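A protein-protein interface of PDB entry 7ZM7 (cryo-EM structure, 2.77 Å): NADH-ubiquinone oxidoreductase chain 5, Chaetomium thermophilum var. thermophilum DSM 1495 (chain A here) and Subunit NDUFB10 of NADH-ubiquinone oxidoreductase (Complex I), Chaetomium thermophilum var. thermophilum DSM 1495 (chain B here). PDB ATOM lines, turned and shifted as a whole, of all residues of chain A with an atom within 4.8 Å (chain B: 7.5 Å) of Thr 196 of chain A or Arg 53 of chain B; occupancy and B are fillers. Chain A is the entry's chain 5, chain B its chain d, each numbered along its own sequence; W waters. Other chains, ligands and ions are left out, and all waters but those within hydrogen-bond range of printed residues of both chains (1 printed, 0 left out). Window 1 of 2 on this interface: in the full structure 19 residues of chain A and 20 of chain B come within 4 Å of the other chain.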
ATOM      1  N   TRP A  69     -13.543 -22.729 -20.949  1.00  0.00           N
ATOM      2  CA  TRP A  69     -13.907 -21.427 -20.394  1.00  0.00           C
ATOM      3  C   TRP A  69     -12.718 -20.552 -20.044  1.00  0.00           C
ATOM      4  O   TRP A  69     -12.882 -19.345 -19.885  1.00  0.00           O
ATOM      5  CB  TRP A  69     -14.757 -21.561 -19.132  1.00  0.00           C
ATOM      6  CG  TRP A  69     -16.190 -21.789 -19.358  1.00  0.00           C
ATOM      7  CD1 TRP A  69     -16.932 -22.778 -18.826  1.00  0.00           C
ATOM      8  CD2 TRP A  69     -17.069 -21.019 -20.168  1.00  0.00           C
ATOM      9  NE1 TRP A  69     -18.218 -22.690 -19.245  1.00  0.00           N
ATOM     10  CE2 TRP A  69     -18.330 -21.612 -20.078  1.00  0.00           C
ATOM     11  CE3 TRP A  69     -16.915 -19.886 -20.962  1.00  0.00           C
ATOM     12  CZ2 TRP A  69     -19.428 -21.117 -20.753  1.00  0.00           C
ATOM     13  CZ3 TRP A  69     -17.997 -19.404 -21.626  1.00  0.00           C
ATOM     14  CH2 TRP A  69     -19.242 -20.011 -21.516  1.00  0.00           C
ATOM     15  N   ILE A  71      -9.467 -19.231 -21.568  1.00  0.00           N
ATOM     16  CA  ILE A  71      -8.521 -19.046 -22.657  1.00  0.00           C
ATOM     17  C   ILE A  71      -7.835 -17.697 -22.461  1.00  0.00           C
ATOM     18  O   ILE A  71      -8.435 -16.635 -22.645  1.00  0.00           O
ATOM     19  CB  ILE A  71      -9.189 -19.198 -24.036  1.00  0.00           C
ATOM     20  CG1 ILE A  71      -8.168 -19.000 -25.149  1.00  0.00           C
ATOM     21  CG2 ILE A  71     -10.397 -18.290 -24.216  1.00  0.00           C
ATOM     22  CD1 ILE A  71      -8.635 -19.449 -26.485  1.00  0.00           C
ATOM     23  N   LEU A 189     -16.991 -15.131 -13.756  1.00  0.00           N
ATOM     24  CA  LEU A 189     -17.230 -14.757 -15.143  1.00  0.00           C
ATOM     25  C   LEU A 189     -16.598 -15.693 -16.155  1.00  0.00           C
ATOM     26  O   LEU A 189     -16.764 -15.480 -17.353  1.00  0.00           O
ATOM     27  CB  LEU A 189     -16.748 -13.324 -15.390  1.00  0.00           C
ATOM     28  CG  LEU A 189     -17.674 -12.331 -14.694  1.00  0.00           C
ATOM     29  CD1 LEU A 189     -17.343 -10.904 -15.002  1.00  0.00           C
ATOM     30  CD2 LEU A 189     -19.123 -12.641 -15.061  1.00  0.00           C
ATOM     31  N   GLY A 190     -15.871 -16.712 -15.720  1.00  0.00           N
ATOM     32  CA  GLY A 190     -15.343 -17.691 -16.642  1.00  0.00           C
ATOM     33  C   GLY A 190     -14.071 -17.269 -17.332  1.00  0.00           C
ATOM     34  O   GLY A 190     -13.234 -18.103 -17.657  1.00  0.00           O
ATOM     35  N   ASN A 191     -13.906 -15.983 -17.564  1.00  0.00           N
ATOM     36  CA  ASN A 191     -12.708 -15.483 -18.200  1.00  0.00           C
ATOM     37  C   ASN A 191     -12.185 -14.287 -17.432  1.00  0.00           C
ATOM     38  O   ASN A 191     -12.877 -13.711 -16.598  1.00  0.00           O
ATOM     39  CB  ASN A 191     -12.947 -15.088 -19.653  1.00  0.00           C
ATOM     40  CG  ASN A 191     -11.764 -15.396 -20.528  1.00  0.00           C
ATOM     41  OD1 ASN A 191     -10.999 -16.314 -20.256  1.00  0.00           O
ATOM     42  ND2 ASN A 191     -11.576 -14.597 -21.557  1.00  0.00           N
ATOM     43  N   ASP A 193     -10.111 -11.826 -19.351  1.00  0.00           N
ATOM     44  CA  ASP A 193      -9.768 -10.744 -20.258  1.00  0.00           C
ATOM     45  C   ASP A 193     -10.416  -9.453 -19.797  1.00  0.00           C
ATOM     46  O   ASP A 193     -11.518  -9.456 -19.257  1.00  0.00           O
ATOM     47  CB  ASP A 193     -10.243 -11.051 -21.673  1.00  0.00           C
ATOM     48  CG  ASP A 193      -9.689 -12.336 -22.208  1.00  0.00           C
ATOM     49  OD1 ASP A 193      -8.885 -12.982 -21.510  1.00  0.00           O
ATOM     50  OD2 ASP A 193     -10.064 -12.713 -23.333  1.00  0.00           O
ATOM     51  N   TYR A 194      -9.727  -8.335 -20.028  1.00  0.00           N
ATOM     52  CA  TYR A 194     -10.219  -7.048 -19.541  1.00  0.00           C
ATOM     53  C   TYR A 194     -11.557  -6.705 -20.155  1.00  0.00           C
ATOM     54  O   TYR A 194     -12.463  -6.231 -19.466  1.00  0.00           O
ATOM     55  CB  TYR A 194      -9.225  -5.937 -19.857  1.00  0.00           C
ATOM     56  CG  TYR A 194      -7.963  -5.982 -19.063  1.00  0.00           C
ATOM     57  CD1 TYR A 194      -7.959  -6.470 -17.779  1.00  0.00           C
ATOM     58  CD2 TYR A 194      -6.777  -5.536 -19.599  1.00  0.00           C
ATOM     59  CE1 TYR A 194      -6.817  -6.515 -17.050  1.00  0.00           C
ATOM     60  CE2 TYR A 194      -5.629  -5.574 -18.876  1.00  0.00           C
ATOM     61  CZ  TYR A 194      -5.652  -6.069 -17.598  1.00  0.00           C
ATOM     62  OH  TYR A 194      -4.507  -6.108 -16.848  1.00  0.00           O
ATOM     63  N   ALA A 195     -11.690  -6.922 -21.460  1.00  0.00           N
ATOM     64  CA  ALA A 195     -12.920  -6.574 -22.145  1.00  0.00           C
ATOM     65  C   ALA A 195     -14.096  -7.335 -21.568  1.00  0.00           C
ATOM     66  O   ALA A 195     -15.173  -6.765 -21.369  1.00  0.00           O
ATOM     67  CB  ALA A 195     -12.774  -6.855 -23.636  1.00  0.00           C
ATOM     68  N   THR A 196     -13.908  -8.626 -21.289  1.00  0.00           N
ATOM     69  CA  THR A 196     -14.966  -9.424 -20.682  1.00  0.00           C
ATOM     70  C   THR A 196     -15.319  -8.905 -19.302  1.00  0.00           C
ATOM     71  O   THR A 196     -16.494  -8.735 -18.972  1.00  0.00           O
ATOM     72  CB  THR A 196     -14.527 -10.885 -20.591  1.00  0.00           C
ATOM     73  OG1 THR A 196     -14.011 -11.319 -21.853  1.00  0.00           O
ATOM     74  CG2 THR A 196     -15.680 -11.777 -20.173  1.00  0.00           C
ATOM     75  N   VAL A 197     -14.312  -8.646 -18.479  1.00  0.00           N
ATOM     76  CA  VAL A 197     -14.567  -8.316 -17.083  1.00  0.00           C
ATOM     77  C   VAL A 197     -15.319  -7.007 -16.983  1.00  0.00           C
ATOM     78  O   VAL A 197     -16.184  -6.834 -16.119  1.00  0.00           O
ATOM     79  CB  VAL A 197     -13.243  -8.286 -16.301  1.00  0.00           C
ATOM     80  CG1 VAL A 197     -13.443  -7.717 -14.919  1.00  0.00           C
ATOM     81  CG2 VAL A 197     -12.661  -9.692 -16.206  1.00  0.00           C
ATOM     82  N   PHE A 198     -15.021  -6.068 -17.877  1.00  0.00           N
ATOM     83  CA  PHE A 198     -15.627  -4.754 -17.782  1.00  0.00           C
ATOM     84  C   PHE A 198     -16.952  -4.686 -18.524  1.00  0.00           C
ATOM     85  O   PHE A 198     -17.861  -3.980 -18.088  1.00  0.00           O
ATOM     86  CB  PHE A 198     -14.649  -3.708 -18.295  1.00  0.00           C
ATOM     87  CG  PHE A 198     -13.306  -3.779 -17.645  1.00  0.00           C
ATOM     88  CD1 PHE A 198     -13.174  -4.224 -16.345  1.00  0.00           C
ATOM     89  CD2 PHE A 198     -12.173  -3.404 -18.329  1.00  0.00           C
ATOM     90  CE1 PHE A 198     -11.943  -4.304 -15.758  1.00  0.00           C
ATOM     91  CE2 PHE A 198     -10.939  -3.479 -17.729  1.00  0.00           C
ATOM     92  CZ  PHE A 198     -10.831  -3.926 -16.448  1.00  0.00           C
ATOM     93  N   SER A 199     -17.102  -5.431 -19.615  1.00  0.00           N
ATOM     94  CA  SER A 199     -18.400  -5.480 -20.268  1.00  0.00           C
ATOM     95  C   SER A 199     -19.465  -6.070 -19.355  1.00  0.00           C
ATOM     96  O   SER A 199     -20.637  -5.713 -19.463  1.00  0.00           O
ATOM     97  CB  SER A 199     -18.311  -6.274 -21.563  1.00  0.00           C
ATOM     98  OG  SER A 199     -17.773  -7.552 -21.330  1.00  0.00           O
ATOM     99  N   LEU A 200     -19.075  -6.940 -18.437  1.00  0.00           N
ATOM    100  CA  LEU A 200     -20.019  -7.674 -17.616  1.00  0.00           C
ATOM    101  C   LEU A 200     -20.180  -7.132 -16.212  1.00  0.00           C
ATOM    102  O   LEU A 200     -21.140  -7.511 -15.542  1.00  0.00           O
ATOM    103  CB  LEU A 200     -19.596  -9.133 -17.516  1.00  0.00           C
ATOM    104  CG  LEU A 200     -19.846  -9.964 -18.753  1.00  0.00           C
ATOM    105  CD1 LEU A 200     -19.426 -11.353 -18.441  1.00  0.00           C
ATOM    106  CD2 LEU A 200     -21.301  -9.914 -19.106  1.00  0.00           C
ATOM    107  N   VAL B  46     -19.491 -25.132 -24.799  1.00  0.00           N
ATOM    108  CA  VAL B  46     -18.540 -24.231 -24.098  1.00  0.00           C
ATOM    109  C   VAL B  46     -17.719 -23.486 -25.147  1.00  0.00           C
ATOM    110  O   VAL B  46     -17.326 -22.332 -24.880  1.00  0.00           O
ATOM    111  CB  VAL B  46     -17.682 -24.970 -23.056  1.00  0.00           C
ATOM    112  CG1 VAL B  46     -16.556 -24.100 -22.523  1.00  0.00           C
ATOM    113  CG2 VAL B  46     -18.527 -25.512 -21.915  1.00  0.00           C
ATOM    114  N   MET B  47     -17.527 -24.090 -26.318  1.00  0.00           N
ATOM    115  CA  MET B  47     -16.863 -23.339 -27.365  1.00  0.00           C
ATOM    116  C   MET B  47     -17.775 -22.318 -28.022  1.00  0.00           C
ATOM    117  O   MET B  47     -17.269 -21.345 -28.580  1.00  0.00           O
ATOM    118  CB  MET B  47     -16.278 -24.264 -28.428  1.00  0.00           C
ATOM    119  CG  MET B  47     -15.159 -25.167 -27.936  1.00  0.00           C
ATOM    120  SD  MET B  47     -13.689 -24.366 -27.302  1.00  0.00           S
ATOM    121  CE  MET B  47     -13.925 -24.543 -25.533  1.00  0.00           C
ATOM    122  N   MET B  48     -19.089 -22.476 -27.850  1.00  0.00           N
ATOM    123  CA  MET B  48     -20.051 -21.458 -28.349  1.00  0.00           C
ATOM    124  C   MET B  48     -19.876 -20.202 -27.496  1.00  0.00           C
ATOM    125  O   MET B  48     -19.926 -19.105 -28.069  1.00  0.00           O
ATOM    126  CB  MET B  48     -21.495 -21.959 -28.253  1.00  0.00           C
ATOM    127  CG  MET B  48     -22.009 -22.565 -29.533  1.00  0.00           C
ATOM    128  SD  MET B  48     -23.590 -23.391 -29.292  1.00  0.00           S
ATOM    129  CE  MET B  48     -24.646 -21.983 -28.958  1.00  0.00           C
ATOM    130  N   GLY B  49     -19.677 -20.359 -26.183  1.00  0.00           N
ATOM    131  CA  GLY B  49     -19.391 -19.224 -25.326  1.00  0.00           C
ATOM    132  C   GLY B  49     -18.081 -18.557 -25.681  1.00  0.00           C
ATOM    133  O   GLY B  49     -17.977 -17.333 -25.684  1.00  0.00           O
ATOM    134  N   ARG B  50     -17.034 -19.348 -25.899  1.00  0.00           N
ATOM    135  CA  ARG B  50     -15.732 -18.786 -26.343  1.00  0.00           C
ATOM    136  C   ARG B  50     -15.944 -17.819 -27.522  1.00  0.00           C
ATOM    137  O   ARG B  50     -15.450 -16.688 -27.436  1.00  0.00           O
ATOM    138  CB  ARG B  50     -14.752 -19.928 -26.619  1.00  0.00           C
ATOM    139  CG  ARG B  50     -13.374 -19.493 -27.091  1.00  0.00           C
ATOM    140  CD  ARG B  50     -12.444 -20.681 -27.232  1.00  0.00           C
ATOM    141  NE  ARG B  50     -11.992 -21.204 -25.951  1.00  0.00           N
ATOM    142  CZ  ARG B  50     -11.130 -22.202 -25.812  1.00  0.00           C
ATOM    143  NH1 ARG B  50     -10.768 -22.607 -24.607  1.00  0.00           N
ATOM    144  NH2 ARG B  50     -10.631 -22.796 -26.878  1.00  0.00           N
ATOM    145  N   LEU B  51     -16.664 -18.235 -28.568  1.00  0.00           N
ATOM    146  CA  LEU B  51     -16.870 -17.406 -29.781  1.00  0.00           C
ATOM    147  C   LEU B  51     -17.704 -16.157 -29.492  1.00  0.00           C
ATOM    148  O   LEU B  51     -17.328 -15.091 -29.992  1.00  0.00           O
ATOM    149  CB  LEU B  51     -17.509 -18.283 -30.857  1.00  0.00           C
ATOM    150  CG  LEU B  51     -16.575 -19.287 -31.526  1.00  0.00           C
ATOM    151  CD1 LEU B  51     -17.333 -20.146 -32.518  1.00  0.00           C
ATOM    152  CD2 LEU B  51     -15.430 -18.570 -32.218  1.00  0.00           C
ATOM    153  N   VAL B  52     -18.780 -16.277 -28.723  1.00  0.00           N
ATOM    154  CA  VAL B  52     -19.601 -15.090 -28.340  1.00  0.00           C
ATOM    155  C   VAL B  52     -18.723 -14.127 -27.539  1.00  0.00           C
ATOM    156  O   VAL B  52     -18.787 -12.928 -27.815  1.00  0.00           O
ATOM    157  CB  VAL B  52     -20.863 -15.504 -27.556  1.00  0.00           C
ATOM    158  CG1 VAL B  52     -21.539 -14.324 -26.878  1.00  0.00           C
ATOM    159  CG2 VAL B  52     -21.854 -16.252 -28.428  1.00  0.00           C
ATOM    160  N   ARG B  53     -17.895 -14.640 -26.623  1.00  0.00           N
ATOM    161  CA  ARG B  53     -16.994 -13.795 -25.793  1.00  0.00           C
ATOM    162  C   ARG B  53     -15.993 -13.082 -26.705  1.00  0.00           C
ATOM    163  O   ARG B  53     -15.697 -11.909 -26.434  1.00  0.00           O
ATOM    164  CB  ARG B  53     -16.360 -14.639 -24.687  1.00  0.00           C
ATOM    165  CG  ARG B  53     -15.555 -13.847 -23.670  1.00  0.00           C
ATOM    166  CD  ARG B  53     -15.056 -14.779 -22.592  1.00  0.00           C
ATOM    167  NE  ARG B  53     -14.353 -15.921 -23.152  1.00  0.00           N
ATOM    168  CZ  ARG B  53     -14.233 -17.094 -22.546  1.00  0.00           C
ATOM    169  NH1 ARG B  53     -13.576 -18.080 -23.130  1.00  0.00           N
ATOM    170  NH2 ARG B  53     -14.785 -17.284 -21.362  1.00  0.00           N
ATOM    171  N   GLU B  54     -15.489 -13.754 -27.736  1.00  0.00           N
ATOM    172  CA  GLU B  54     -14.601 -13.105 -28.737  1.00  0.00           C
ATOM    173  C   GLU B  54     -15.353 -11.997 -29.482  1.00  0.00           C
ATOM    174  O   GLU B  54     -14.739 -10.963 -29.765  1.00  0.00           O
ATOM    175  CB  GLU B  54     -14.102 -14.128 -29.752  1.00  0.00           C
ATOM    176  CG  GLU B  54     -13.152 -15.153 -29.165  1.00  0.00           C
ATOM    177  CD  GLU B  54     -12.757 -16.263 -30.121  1.00  0.00           C
ATOM    178  OE1 GLU B  54     -13.225 -16.238 -31.276  1.00  0.00           O
ATOM    179  OE2 GLU B  54     -11.980 -17.147 -29.710  1.00  0.00           O
ATOM    180  N   GLU B  55     -16.617 -12.211 -29.842  1.00  0.00           N
ATOM    181  CA  GLU B  55     -17.383 -11.102 -30.468  1.00  0.00           C
ATOM    182  C   GLU B  55     -17.576  -9.972 -29.450  1.00  0.00           C
ATOM    183  O   GLU B  55     -17.399  -8.806 -29.832  1.00  0.00           O
ATOM    184  CB  GLU B  55     -18.700 -11.616 -31.048  1.00  0.00           C
ATOM    185  CG  GLU B  55     -18.521 -12.607 -32.181  1.00  0.00           C
ATOM    186  CD  GLU B  55     -18.185 -11.996 -33.531  1.00  0.00           C
ATOM    187  OE1 GLU B  55     -17.652 -12.723 -34.392  1.00  0.00           O
ATOM    188  OE2 GLU B  55     -18.470 -10.797 -33.726  1.00  0.00           O
ATOM    189  N   LEU B  56     -17.915 -10.308 -28.205  1.00  0.00           N
ATOM    190  CA  LEU B  56     -18.150  -9.280 -27.160  1.00  0.00           C
ATOM    191  C   LEU B  56     -16.890  -8.436 -27.035  1.00  0.00           C
ATOM    192  O   LEU B  56     -17.009  -7.221 -26.919  1.00  0.00           O
ATOM    193  CB  LEU B  56     -18.474  -9.970 -25.833  1.00  0.00           C
ATOM    194  CG  LEU B  56     -19.003  -9.084 -24.708  1.00  0.00           C
ATOM    195  CD1 LEU B  56     -20.116  -8.180 -25.205  1.00  0.00           C
ATOM    196  CD2 LEU B  56     -19.488  -9.932 -23.543  1.00  0.00           C
ATOM    197  N   SER B  57     -15.726  -9.080 -27.072  1.00  0.00           N
ATOM    198  CA  SER B  57     -14.484  -8.336 -26.923  1.00  0.00           C
ATOM    199  C   SER B  57     -14.326  -7.300 -28.020  1.00  0.00           C
ATOM    200  O   SER B  57     -13.985  -6.147 -27.742  1.00  0.00           O
ATOM    201  CB  SER B  57     -13.300  -9.291 -26.918  1.00  0.00           C
ATOM    202  OG  SER B  57     -13.152  -9.915 -28.178  1.00  0.00           O
ATOM    203  N   LYS B  58     -14.583  -7.680 -29.270  1.00  0.00           N
ATOM    204  CA  LYS B  58     -14.500  -6.714 -30.355  1.00  0.00           C
ATOM    205  C   LYS B  58     -15.542  -5.616 -30.207  1.00  0.00           C
ATOM    206  O   LYS B  58     -15.245  -4.442 -30.438  1.00  0.00           O
ATOM    207  CB  LYS B  58     -14.633  -7.418 -31.699  1.00  0.00           C
ATOM    208  CG  LYS B  58     -13.466  -8.319 -31.995  1.00  0.00           C
ATOM    209  CD  LYS B  58     -13.519  -8.883 -33.397  1.00  0.00           C
ATOM    210  CE  LYS B  58     -14.573  -9.948 -33.513  1.00  0.00           C
ATOM    211  NZ  LYS B  58     -14.559 -10.588 -34.857  1.00  0.00           N
ATOM    212  N   CYS B  59     -16.769  -5.970 -29.820  1.00  0.00           N
ATOM    213  CA  CYS B  59     -17.785  -4.947 -29.600  1.00  0.00           C
ATOM    214  C   CYS B  59     -17.360  -3.986 -28.502  1.00  0.00           C
ATOM    215  O   CYS B  59     -17.608  -2.782 -28.595  1.00  0.00           O
ATOM    216  CB  CYS B  59     -19.125  -5.592 -29.254  1.00  0.00           C
ATOM    217  SG  CYS B  59     -20.541  -4.438 -29.218  1.00  0.00           S
ATOM    218  N   TYR B  60     -16.710  -4.497 -27.460  1.00  0.00           N
ATOM    219  CA  TYR B  60     -16.263  -3.640 -26.369  1.00  0.00           C
ATOM    220  C   TYR B  60     -15.257  -2.608 -26.853  1.00  0.00           C
ATOM    221  O   TYR B  60     -15.400  -1.415 -26.579  1.00  0.00           O
ATOM    222  CB  TYR B  60     -15.652  -4.491 -25.260  1.00  0.00           C
ATOM    223  CG  TYR B  60     -15.172  -3.700 -24.069  1.00  0.00           C
ATOM    224  CD1 TYR B  60     -13.880  -3.194 -24.017  1.00  0.00           C
ATOM    225  CD2 TYR B  60     -16.007  -3.464 -23.002  1.00  0.00           C
ATOM    226  CE1 TYR B  60     -13.449  -2.469 -22.943  1.00  0.00           C
ATOM    227  CE2 TYR B  60     -15.577  -2.758 -21.923  1.00  0.00           C
ATOM    228  CZ  TYR B  60     -14.303  -2.255 -21.897  1.00  0.00           C
ATOM    229  OH  TYR B  60     -13.895  -1.544 -20.809  1.00  0.00           O
ATOM    230  N   TYR B  61     -14.231  -3.049 -27.571  1.00  0.00           N
ATOM    231  CA  TYR B  61     -13.213  -2.129 -28.059  1.00  0.00           C
ATOM    232  C   TYR B  61     -13.698  -1.273 -29.211  1.00  0.00           C
ATOM    233  O   TYR B  61     -13.143  -0.197 -29.437  1.00  0.00           O
ATOM    234  CB  TYR B  61     -11.962  -2.899 -28.468  1.00  0.00           C
ATOM    235  CG  TYR B  61     -11.238  -3.397 -27.259  1.00  0.00           C
ATOM    236  CD1 TYR B  61     -10.820  -2.519 -26.282  1.00  0.00           C
ATOM    237  CD2 TYR B  61     -11.023  -4.737 -27.061  1.00  0.00           C
ATOM    238  CE1 TYR B  61     -10.189  -2.963 -25.163  1.00  0.00           C
ATOM    239  CE2 TYR B  61     -10.399  -5.187 -25.940  1.00  0.00           C
ATOM    240  CZ  TYR B  61      -9.982  -4.299 -24.998  1.00  0.00           C
ATOM    241  OH  TYR B  61      -9.343  -4.752 -23.869  1.00  0.00           O
ATOM    242  N   LEU B  74     -24.994  -9.568 -27.102  1.00  0.00           N
ATOM    243  CA  LEU B  74     -23.854 -10.447 -26.889  1.00  0.00           C
ATOM    244  C   LEU B  74     -23.660 -10.732 -25.413  1.00  0.00           C
ATOM    245  O   LEU B  74     -23.289 -11.846 -25.031  1.00  0.00           O
ATOM    246  CB  LEU B  74     -22.591  -9.832 -27.473  1.00  0.00           C
ATOM    247  CG  LEU B  74     -22.362 -10.020 -28.963  1.00  0.00           C
ATOM    248  CD1 LEU B  74     -21.213  -9.148 -29.398  1.00  0.00           C
ATOM    249  CD2 LEU B  74     -22.078 -11.469 -29.272  1.00  0.00           C
ATOM    250  N   ARG B  75     -23.894  -9.737 -24.566  1.00  0.00           N
ATOM    251  CA  ARG B  75     -23.796  -9.969 -23.134  1.00  0.00           C
ATOM    252  C   ARG B  75     -24.820 -10.988 -22.675  1.00  0.00           C
ATOM    253  O   ARG B  75     -24.508 -11.875 -21.875  1.00  0.00           O
ATOM    254  CB  ARG B  75     -23.986  -8.665 -22.374  1.00  0.00           C
ATOM    255  CG  ARG B  75     -22.776  -7.807 -22.319  1.00  0.00           C
ATOM    256  CD  ARG B  75     -22.931  -6.797 -21.248  1.00  0.00           C
ATOM    257  NE  ARG B  75     -24.123  -5.992 -21.451  1.00  0.00           N
ATOM    258  CZ  ARG B  75     -24.120  -4.752 -21.921  1.00  0.00           C
ATOM    259  NH1 ARG B  75     -25.261  -4.101 -22.057  1.00  0.00           N
ATOM    260  NH2 ARG B  75     -22.980  -4.164 -22.248  1.00  0.00           N
ATOM    261  N   ARG B  77     -26.331 -13.406 -24.416  1.00  0.00           N
ATOM    262  CA  ARG B  77     -26.013 -14.772 -24.908  1.00  0.00           C
ATOM    263  C   ARG B  77     -24.861 -15.348 -24.087  1.00  0.00           C
ATOM    264  O   ARG B  77     -24.943 -16.527 -23.713  1.00  0.00           O
ATOM    265  CB  ARG B  77     -25.628 -14.758 -26.389  1.00  0.00           C
ATOM    266  CG  ARG B  77     -25.579 -16.141 -27.023  1.00  0.00           C
ATOM    267  CD  ARG B  77     -26.965 -16.743 -27.141  1.00  0.00           C
ATOM    268  NE  ARG B  77     -26.929 -18.174 -27.407  1.00  0.00           N
ATOM    269  CZ  ARG B  77     -27.082 -19.112 -26.481  1.00  0.00           C
ATOM    270  NH1 ARG B  77     -27.033 -20.389 -26.819  1.00  0.00           N
ATOM    271  NH2 ARG B  77     -27.293 -18.772 -25.222  1.00  0.00           N
ATOM    272  N   TYR B  78     -23.828 -14.540 -23.821  1.00  0.00           N
ATOM    273  CA  TYR B  78     -22.664 -15.045 -23.103  1.00  0.00           C
ATOM    274  C   TYR B  78     -23.010 -15.397 -21.669  1.00  0.00           C
ATOM    275  O   TYR B  78     -22.496 -16.378 -21.121  1.00  0.00           O
ATOM    276  CB  TYR B  78     -21.535 -14.028 -23.141  1.00  0.00           C
ATOM    277  CG  TYR B  78     -20.361 -14.433 -22.300  1.00  0.00           C
ATOM    278  CD1 TYR B  78     -19.573 -15.527 -22.646  1.00  0.00           C
ATOM    279  CD2 TYR B  78     -20.050 -13.741 -21.148  1.00  0.00           C
ATOM    280  CE1 TYR B  78     -18.515 -15.910 -21.863  1.00  0.00           C
ATOM    281  CE2 TYR B  78     -19.001 -14.119 -20.365  1.00  0.00           C
ATOM    282  CZ  TYR B  78     -18.233 -15.194 -20.719  1.00  0.00           C
ATOM    283  OH  TYR B  78     -17.177 -15.543 -19.920  1.00  0.00           O
ATOM    284  N   LEU B  81     -24.867 -18.829 -21.669  1.00  0.00           N
ATOM    285  CA  LEU B  81     -23.973 -19.966 -21.819  1.00  0.00           C
ATOM    286  C   LEU B  81     -23.125 -20.183 -20.574  1.00  0.00           C
ATOM    287  O   LEU B  81     -22.762 -21.318 -20.267  1.00  0.00           O
ATOM    288  CB  LEU B  81     -23.092 -19.767 -23.045  1.00  0.00           C
ATOM    289  CG  LEU B  81     -23.777 -19.764 -24.419  1.00  0.00           C
ATOM    290  CD1 LEU B  81     -23.095 -18.779 -25.313  1.00  0.00           C
ATOM    291  CD2 LEU B  81     -23.774 -21.137 -25.081  1.00  0.00           C
ATOM    292  N   LEU B  82     -22.823 -19.121 -19.834  1.00  0.00           N
ATOM    293  CA  LEU B  82     -21.974 -19.258 -18.660  1.00  0.00           C
ATOM    294  C   LEU B  82     -22.673 -19.988 -17.520  1.00  0.00           C
ATOM    295  O   LEU B  82     -22.009 -20.511 -16.621  1.00  0.00           O
ATOM    296  CB  LEU B  82     -21.511 -17.879 -18.208  1.00  0.00           C
ATOM    297  CG  LEU B  82     -20.408 -17.825 -17.163  1.00  0.00           C
ATOM    298  CD1 LEU B  82     -19.162 -18.577 -17.612  1.00  0.00           C
ATOM    299  CD2 LEU B  82     -20.114 -16.381 -16.856  1.00  0.00           C
HETATM  300  O   HOH W   1     -20.261 -22.279 -16.880  1.00  0.00           O
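The guanidinium group (NH2) of Arg 53 of chain B sits at hydrogen-bond distance from the backbone carbonyl oxygen (O) of Trp 69 of chain A, at 3.2 Å. The backbone carbonyl oxygen (O) of Leu 189 of chain A lies within hydrogen-bond range of the side-chain hydroxyl (OH) of Tyr 78 of chain B (2.6 Å). The guanidinium group (NE) of Arg 53 of chain B sits close to the side-chain amide nitrogen (ND2) of Asn 191 of chain A.
The backbone carbonyl oxygen (O) of Thr 196 of chain A is in hydrogen-bond range of the side-chain hydroxyl (OG) of Ser 199 of chain A (2.9 Å). The backbone carbonyl oxygen (O) of Glu 54 of chain B sits at hydrogen-bond distance from the side-chain hydroxyl (OG) of Ser 57 of chain B. The side-chain sulfur (SD) of Met 47 of chain B sits at hydrogen-bond distance from the guanidinium group (NH2) of Arg 50 of chain B (3.5 Å). The backbone carbonyl oxygen of Ala 195 of chain A lies within hydrogen-bond range of the side-chain hydroxyl of Ser 199 of chain A, 2.7 Å away. The side-chain amide nitrogen of Asn 191 of chain A sits at hydrogen-bond distance from the side-chain carboxylate of Asp 193 of chain A (3.0 Å). NH2 of Arg 53 of chain B is in hydrogen-bond range of OH of Tyr 78 of chain B, at 3.3 Å.
Among the printed residues, merely in contact across the chains: Trp 69 of chain A with Val 46 of chain B, Trp 69 of chain A with Gly 49 of chain B, Trp 69 of chain A with Tyr 78 of chain B, Trp 69 of chain A with Leu 81 of chain B, Trp 69 of chain A with Leu 82 of chain B, Ile 71 of chain A with Arg 50 of chain B, Ile 71 of chain A with Arg 53 of chain B, Leu 189 of chain A with Leu 82 of chain B, Ala 195 of chain A with Ser 57 of chain B, Ala 195 of chain A with Tyr 60 of chain B, Ala 195 of chain A with Tyr 61 of chain B, Thr 196 of chain A with Arg 53 of chain B, Phe 198 of chain A with Tyr 60 of chain B, Ser 199 of chain A with Leu 56 of chain B, Ser 199 of chain A with Tyr 60 of chain B, Ser 199 of chain A with Arg 75 of chain B and Leu 200 of chain A with Tyr 78 of chain B.
Thr 196 of chain A touches just one residue of chain B: Arg 53 (3.5 Å). Leu 51 of chain B touches none of the printed residues of chain A. Of chain A, only Trp 69 (3.2 Å), Ile 71 (3.4 Å), Asn 191 (3.3 Å) and Thr 196 (3.5 Å) come within 4 Å of Arg 53 of chain B. Of the printed residues of chain A, Tyr 60 of chain B touches Ala 195 (3.8 Å), Phe 198 (3.4 Å) and Ser 199 (3.8 Å). Of the printed residues of chain A, Leu 82 of chain B touches Trp 69 and Leu 189. The nearest residue of chain B that does not touch Thr 196 of chain A is Tyr 78 of chain B (4.1 Å). The nearest residue of chain A that does not touch Arg 53 of chain B is Gly 190 of chain A (4.1 Å). The nearest printed residue of chain A that does not touch Ser 57 of chain B is Thr 196 of chain A (5.5 Å).
Along chain B the printed residues that touch a printed residue of chain A span positions 46 to 82. Of the 13 printed residues of chain A, 9 touch a printed residue of chain B. Hydrophobic or aromatic side chains of chain A within 4 Å of the printed part of chain B: Trp 69, Ile 71, Ala 195, Phe 198 and Leu 200. Along chain A the printed residues that touch a printed residue of chain B span positions 69 to 200. Among the printed residues, 20 pairs touch across the chains.
Water W1 bridges O of Leu 82 of chain B (2.5 Å) and NE1 of Trp 69 of chain A (3.2 Å).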
